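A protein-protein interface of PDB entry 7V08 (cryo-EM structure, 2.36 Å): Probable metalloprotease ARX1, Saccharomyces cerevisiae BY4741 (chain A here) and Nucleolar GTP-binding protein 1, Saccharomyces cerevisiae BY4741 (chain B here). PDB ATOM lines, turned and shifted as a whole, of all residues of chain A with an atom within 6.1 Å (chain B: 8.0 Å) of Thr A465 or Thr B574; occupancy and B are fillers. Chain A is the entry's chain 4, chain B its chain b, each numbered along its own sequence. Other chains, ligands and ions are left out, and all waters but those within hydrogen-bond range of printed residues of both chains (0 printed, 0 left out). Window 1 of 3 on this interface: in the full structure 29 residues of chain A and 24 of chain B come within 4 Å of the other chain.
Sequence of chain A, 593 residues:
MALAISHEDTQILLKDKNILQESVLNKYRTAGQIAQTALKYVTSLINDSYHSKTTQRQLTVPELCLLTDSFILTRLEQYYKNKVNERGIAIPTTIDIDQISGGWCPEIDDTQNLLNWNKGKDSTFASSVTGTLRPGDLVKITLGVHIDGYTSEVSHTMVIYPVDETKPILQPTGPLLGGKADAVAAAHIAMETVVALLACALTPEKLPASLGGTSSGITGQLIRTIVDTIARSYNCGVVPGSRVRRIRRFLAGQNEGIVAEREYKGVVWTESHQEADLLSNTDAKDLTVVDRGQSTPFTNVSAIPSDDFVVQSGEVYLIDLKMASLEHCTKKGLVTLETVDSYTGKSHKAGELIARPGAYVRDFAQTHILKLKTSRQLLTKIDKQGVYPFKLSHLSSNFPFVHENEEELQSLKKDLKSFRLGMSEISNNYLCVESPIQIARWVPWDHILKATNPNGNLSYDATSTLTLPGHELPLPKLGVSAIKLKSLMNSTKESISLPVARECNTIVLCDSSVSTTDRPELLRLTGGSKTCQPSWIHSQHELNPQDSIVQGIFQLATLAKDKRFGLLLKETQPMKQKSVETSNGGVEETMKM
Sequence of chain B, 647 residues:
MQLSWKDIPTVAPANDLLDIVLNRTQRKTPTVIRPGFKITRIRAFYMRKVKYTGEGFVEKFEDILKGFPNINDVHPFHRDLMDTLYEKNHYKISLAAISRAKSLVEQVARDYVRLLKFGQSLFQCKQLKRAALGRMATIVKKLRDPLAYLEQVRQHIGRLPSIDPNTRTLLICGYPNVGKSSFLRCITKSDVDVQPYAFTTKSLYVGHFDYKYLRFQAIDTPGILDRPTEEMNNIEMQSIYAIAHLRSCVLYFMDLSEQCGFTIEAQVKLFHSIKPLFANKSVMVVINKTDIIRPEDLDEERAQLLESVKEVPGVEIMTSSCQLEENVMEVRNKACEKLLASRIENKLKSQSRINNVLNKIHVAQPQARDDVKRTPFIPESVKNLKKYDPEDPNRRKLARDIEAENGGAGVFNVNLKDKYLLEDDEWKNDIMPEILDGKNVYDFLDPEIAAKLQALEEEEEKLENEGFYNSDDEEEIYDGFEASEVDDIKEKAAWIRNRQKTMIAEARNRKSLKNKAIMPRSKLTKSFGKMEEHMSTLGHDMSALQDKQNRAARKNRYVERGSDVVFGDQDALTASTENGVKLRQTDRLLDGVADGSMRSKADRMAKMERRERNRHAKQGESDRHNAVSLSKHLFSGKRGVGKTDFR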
ATOM      1  N   ASP A 363      -2.900  23.010 -16.966  1.00  0.00           N
ATOM      2  CA  ASP A 363      -3.691  23.069 -15.740  1.00  0.00           C
ATOM      3  C   ASP A 363      -3.857  21.648 -15.218  1.00  0.00           C
ATOM      4  O   ASP A 363      -4.710  20.896 -15.694  1.00  0.00           O
ATOM      5  CB  ASP A 363      -5.040  23.728 -16.004  1.00  0.00           C
ATOM      6  CG  ASP A 363      -5.939  23.730 -14.781  1.00  0.00           C
ATOM      7  OD1 ASP A 363      -5.422  23.764 -13.647  1.00  0.00           O
ATOM      8  OD2 ASP A 363      -7.171  23.693 -14.957  1.00  0.00           O
ATOM      9  N   TYR A 430     -10.208  22.602 -21.986  1.00  0.00           N
ATOM     10  CA  TYR A 430      -9.682  23.384 -20.864  1.00  0.00           C
ATOM     11  C   TYR A 430      -8.532  22.689 -20.139  1.00  0.00           C
ATOM     12  O   TYR A 430      -8.316  22.923 -18.948  1.00  0.00           O
ATOM     13  CB  TYR A 430     -10.790  23.741 -19.863  1.00  0.00           C
ATOM     14  CG  TYR A 430     -12.020  24.355 -20.493  1.00  0.00           C
ATOM     15  CD1 TYR A 430     -11.992  25.640 -21.016  1.00  0.00           C
ATOM     16  CD2 TYR A 430     -13.215  23.652 -20.547  1.00  0.00           C
ATOM     17  CE1 TYR A 430     -13.119  26.201 -21.585  1.00  0.00           C
ATOM     18  CE2 TYR A 430     -14.346  24.206 -21.112  1.00  0.00           C
ATOM     19  CZ  TYR A 430     -14.290  25.479 -21.633  1.00  0.00           C
ATOM     20  OH  TYR A 430     -15.413  26.033 -22.198  1.00  0.00           O
ATOM     21  N   CYS A 432      -5.267  22.956 -21.236  1.00  0.00           N
ATOM     22  CA  CYS A 432      -4.222  23.967 -21.278  1.00  0.00           C
ATOM     23  C   CYS A 432      -4.835  25.325 -21.581  1.00  0.00           C
ATOM     24  O   CYS A 432      -5.950  25.422 -22.100  1.00  0.00           O
ATOM     25  CB  CYS A 432      -3.148  23.658 -22.325  1.00  0.00           C
ATOM     26  SG  CYS A 432      -2.152  22.186 -22.007  1.00  0.00           S
ATOM     27  N   VAL A 433      -4.090  26.377 -21.248  1.00  0.00           N
ATOM     28  CA  VAL A 433      -4.506  27.749 -21.493  1.00  0.00           C
ATOM     29  C   VAL A 433      -3.353  28.499 -22.151  1.00  0.00           C
ATOM     30  O   VAL A 433      -2.200  28.076 -22.108  1.00  0.00           O
ATOM     31  CB  VAL A 433      -4.956  28.463 -20.203  1.00  0.00           C
ATOM     32  CG1 VAL A 433      -6.252  27.860 -19.686  1.00  0.00           C
ATOM     33  CG2 VAL A 433      -3.876  28.362 -19.152  1.00  0.00           C
ATOM     34  N   THR A 463     -17.670  35.618 -20.498  1.00  0.00           N
ATOM     35  CA  THR A 463     -17.144  34.828 -21.602  1.00  0.00           C
ATOM     36  C   THR A 463     -15.640  34.630 -21.514  1.00  0.00           C
ATOM     37  O   THR A 463     -15.067  33.964 -22.380  1.00  0.00           O
ATOM     38  CB  THR A 463     -17.488  35.476 -22.947  1.00  0.00           C
ATOM     39  OG1 THR A 463     -16.939  36.800 -23.002  1.00  0.00           O
ATOM     40  CG2 THR A 463     -18.997  35.552 -23.139  1.00  0.00           C
ATOM     41  N   SER A 464     -14.992  35.201 -20.503  1.00  0.00           N
ATOM     42  CA  SER A 464     -13.558  35.031 -20.330  1.00  0.00           C
ATOM     43  C   SER A 464     -13.247  33.601 -19.916  1.00  0.00           C
ATOM     44  O   SER A 464     -13.945  33.019 -19.080  1.00  0.00           O
ATOM     45  CB  SER A 464     -13.027  36.014 -19.286  1.00  0.00           C
ATOM     46  OG  SER A 464     -11.648  35.800 -19.036  1.00  0.00           O
ATOM     47  N   THR A 465     -12.195  33.033 -20.502  1.00  0.00           N
ATOM     48  CA  THR A 465     -11.817  31.664 -20.178  1.00  0.00           C
ATOM     49  C   THR A 465     -11.156  31.557 -18.807  1.00  0.00           C
ATOM     50  O   THR A 465     -11.460  30.629 -18.054  1.00  0.00           O
ATOM     51  CB  THR A 465     -10.884  31.106 -21.255  1.00  0.00           C
ATOM     52  OG1 THR A 465      -9.644  31.819 -21.221  1.00  0.00           O
ATOM     53  CG2 THR A 465     -11.503  31.277 -22.620  1.00  0.00           C
ATOM     54  N   LEU A 466     -10.265  32.483 -18.466  1.00  0.00           N
ATOM     55  CA  LEU A 466      -9.533  32.440 -17.209  1.00  0.00           C
ATOM     56  C   LEU A 466     -10.300  33.186 -16.125  1.00  0.00           C
ATOM     57  O   LEU A 466     -10.774  34.305 -16.342  1.00  0.00           O
ATOM     58  CB  LEU A 466      -8.136  33.045 -17.360  1.00  0.00           C
ATOM     59  CG  LEU A 466      -7.099  32.372 -18.269  1.00  0.00           C
ATOM     60  CD1 LEU A 466      -5.838  33.214 -18.387  1.00  0.00           C
ATOM     61  CD2 LEU A 466      -6.773  30.967 -17.811  1.00  0.00           C
ATOM     62  N   THR A 467     -10.402  32.563 -14.949  1.00  0.00           N
ATOM     63  CA  THR A 467     -11.160  33.158 -13.855  1.00  0.00           C
ATOM     64  C   THR A 467     -10.430  34.353 -13.249  1.00  0.00           C
ATOM     65  O   THR A 467     -11.064  35.334 -12.843  1.00  0.00           O
ATOM     66  CB  THR A 467     -11.447  32.107 -12.779  1.00  0.00           C
ATOM     67  OG1 THR A 467     -12.228  31.043 -13.337  1.00  0.00           O
ATOM     68  CG2 THR A 467     -12.217  32.731 -11.624  1.00  0.00           C
ATOM     69  N   ASP B 571      -7.903  24.270  -7.753  1.00  0.00           N
ATOM     70  CA  ASP B 571      -8.841  23.688  -8.699  1.00  0.00           C
ATOM     71  C   ASP B 571      -9.058  24.681  -9.830  1.00  0.00           C
ATOM     72  O   ASP B 571      -8.304  25.644  -9.992  1.00  0.00           O
ATOM     73  CB  ASP B 571     -10.163  23.321  -8.020  1.00  0.00           C
ATOM     74  CG  ASP B 571     -11.126  22.623  -8.963  1.00  0.00           C
ATOM     75  OD1 ASP B 571     -10.759  22.408 -10.135  1.00  0.00           O
ATOM     76  OD2 ASP B 571     -12.244  22.270  -8.529  1.00  0.00           O
ATOM     77  N   ALA B 572     -10.084  24.407 -10.633  1.00  0.00           N
ATOM     78  CA  ALA B 572     -10.604  25.331 -11.634  1.00  0.00           C
ATOM     79  C   ALA B 572      -9.555  25.746 -12.653  1.00  0.00           C
ATOM     80  O   ALA B 572      -9.246  24.987 -13.575  1.00  0.00           O
ATOM     81  CB  ALA B 572     -11.193  26.573 -10.954  1.00  0.00           C
ATOM     82  N   LEU B 573      -9.003  26.948 -12.482  1.00  0.00           N
ATOM     83  CA  LEU B 573      -8.148  27.663 -13.428  1.00  0.00           C
ATOM     84  C   LEU B 573      -8.855  27.943 -14.748  1.00  0.00           C
ATOM     85  O   LEU B 573      -8.191  28.295 -15.727  1.00  0.00           O
ATOM     86  CB  LEU B 573      -6.830  26.932 -13.715  1.00  0.00           C
ATOM     87  CG  LEU B 573      -5.921  27.589 -14.750  1.00  0.00           C
ATOM     88  CD1 LEU B 573      -5.480  28.956 -14.245  1.00  0.00           C
ATOM     89  CD2 LEU B 573      -4.729  26.705 -15.067  1.00  0.00           C
ATOM     90  N   THR B 574     -10.171  27.778 -14.816  1.00  0.00           N
ATOM     91  CA  THR B 574     -10.953  28.111 -15.998  1.00  0.00           C
ATOM     92  C   THR B 574     -12.370  28.391 -15.525  1.00  0.00           C
ATOM     93  O   THR B 574     -12.875  27.689 -14.642  1.00  0.00           O
ATOM     94  CB  THR B 574     -10.901  26.976 -17.038  1.00  0.00           C
ATOM     95  OG1 THR B 574      -9.544  26.774 -17.450  1.00  0.00           O
ATOM     96  CG2 THR B 574     -11.765  27.270 -18.256  1.00  0.00           C
ATOM     97  N   ALA B 575     -12.974  29.451 -16.060  1.00  0.00           N
ATOM     98  CA  ALA B 575     -14.327  29.825 -15.668  1.00  0.00           C
ATOM     99  C   ALA B 575     -15.310  28.727 -16.046  1.00  0.00           C
ATOM    100  O   ALA B 575     -15.360  28.300 -17.201  1.00  0.00           O
ATOM    101  CB  ALA B 575     -14.719  31.144 -16.332  1.00  0.00           C
ATOM    102  N   SER B 576     -16.077  28.257 -15.067  1.00  0.00           N
ATOM    103  CA  SER B 576     -17.072  27.230 -15.332  1.00  0.00           C
ATOM    104  C   SER B 576     -18.219  27.815 -16.142  1.00  0.00           C
ATOM    105  O   SER B 576     -18.804  28.834 -15.764  1.00  0.00           O
ATOM    106  CB  SER B 576     -17.593  26.639 -14.025  1.00  0.00           C
ATOM    107  OG  SER B 576     -18.212  27.634 -13.230  1.00  0.00           O
ATOM    108  N   THR B 577     -18.539  27.168 -17.256  1.00  0.00           N
ATOM    109  CA  THR B 577     -19.585  27.654 -18.137  1.00  0.00           C
ATOM    110  C   THR B 577     -20.962  27.389 -17.535  1.00  0.00           C
ATOM    111  O   THR B 577     -21.142  26.531 -16.668  1.00  0.00           O
ATOM    112  CB  THR B 577     -19.470  27.006 -19.515  1.00  0.00           C
ATOM    113  OG1 THR B 577     -19.606  25.587 -19.392  1.00  0.00           O
ATOM    114  CG2 THR B 577     -18.116  27.322 -20.138  1.00  0.00           C
ATOM    115  N   VAL B 581     -20.442  23.917 -21.613  1.00  0.00           N
ATOM    116  CA  VAL B 581     -20.011  23.922 -22.997  1.00  0.00           C
ATOM    117  C   VAL B 581     -18.489  23.845 -23.062  1.00  0.00           C
ATOM    118  O   VAL B 581     -17.781  24.158 -22.105  1.00  0.00           O
ATOM    119  CB  VAL B 581     -20.544  25.172 -23.738  1.00  0.00           C
ATOM    120  CG1 VAL B 581     -22.028  25.331 -23.489  1.00  0.00           C
ATOM    121  CG2 VAL B 581     -19.806  26.428 -23.294  1.00  0.00           C
ATOM    122  N   LEU B 583     -14.804  24.934 -25.221  1.00  0.00           N
ATOM    123  CA  LEU B 583     -14.215  26.244 -25.490  1.00  0.00           C
ATOM    124  C   LEU B 583     -14.835  26.914 -26.711  1.00  0.00           C
ATOM    125  O   LEU B 583     -15.158  28.106 -26.676  1.00  0.00           O
ATOM    126  CB  LEU B 583     -12.704  26.113 -25.673  1.00  0.00           C
ATOM    127  CG  LEU B 583     -11.976  27.414 -26.013  1.00  0.00           C
ATOM    128  CD1 LEU B 583     -12.122  28.395 -24.878  1.00  0.00           C
ATOM    129  CD2 LEU B 583     -10.514  27.173 -26.320  1.00  0.00           C
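The side-chain hydroxyl (OG1) of Thr B577 lies within hydrogen-bond range of the backbone NH (N) of Val B581 (2.9 Å).
The backbone carbonyl oxygen (O) of Leu A466 lies within hydrogen-bond range of the side-chain hydroxyl (OG) of Ser A464 (3.2 Å).
Thr A465 touches just these residues of chain B: Thr B574 (3.3 Å), Ala B575 (2.8 Å) and Leu B583 (3.7 Å).
Thr B574 touches three residues of chain A.
Of chain B, only Ala B575 comes within 4 Å of Ser A464.
Of the printed residues of chain A, Thr B577 touches Tyr A430.
Printed residues of chain B within 4 Å of Asp A363: Ala B572 (2.8 Å) and Leu B573 (3.1 Å).
Printed residues of chain A within 4 Å of Leu B583: Tyr A430 and Thr A465.
Of the printed residues of chain A, Leu B573 touches Asp A363 (3.1 Å) and Leu A466 (3.7 Å).
Of the printed residues of chain B, Thr A467 touches Thr B574 (3.4 Å) and Ala B575 (3.2 Å).
Ser B576 touches none of the printed residues of chain A.
Thr A463 touches none of the printed residues of chain B.
The nearest printed residue of chain A that does not touch Thr B577 is Ser A464 (7.1 Å).
Asp A363 touches Leu B573.
Thr B574 touches Tyr A430 (CG2 to CD1, 3.2 Å).
Tyr A430 touches Thr B577.
Ser A464 touches Ala B575.
Thr B574 touches Thr A465 (CA to O, 3.3 Å).
Leu B583 touches Thr A465 (CD1 to CG2, 3.7 Å).
Leu A466 touches Leu B573 (CD2 to O, 3.7 Å).
Thr A467 touches Thr B574 (OG1 to C, 3.4 Å).
OD2 of Asp A363 sits close to O of Ala B572, at 2.8 Å.
The side-chain hydroxyl of Tyr A430 lies within hydrogen-bond range of the backbone carbonyl oxygen of Val B581 (3.0 Å).
The side-chain hydroxyl of Tyr A430 is in hydrogen-bond range of the backbone NH of Leu B583 (3.3 Å).
The backbone NH of Ala B575 is in hydrogen-bond range of the backbone carbonyl oxygen of Thr A465 (2.8 Å).
The backbone NH (N) of Ala B575 lies within hydrogen-bond range of the side-chain hydroxyl (OG1) of Thr A467 (3.2 Å).
Along chain A the printed residues that touch a printed residue of chain B span positions 363 to 467.
Of the 9 printed residues of chain B, 7 touch a printed residue of chain A.
Printed residues of chain B that touch a printed residue of chain A: Ala B572, Leu B573, Thr B574, Ala B575, Thr B577, Val B581 and Leu B583.
Hydrophobic or aromatic side chains of chain B within 4 Å of the printed part of chain A: Leu B573, Ala B575 and Leu B583.
Among the printed residues, 13 pairs touch across the chains.
Among the printed residues, no Asp or Glu carboxylate lies within 4 Å of a Lys or Arg side-chain nitrogen of the other chain.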
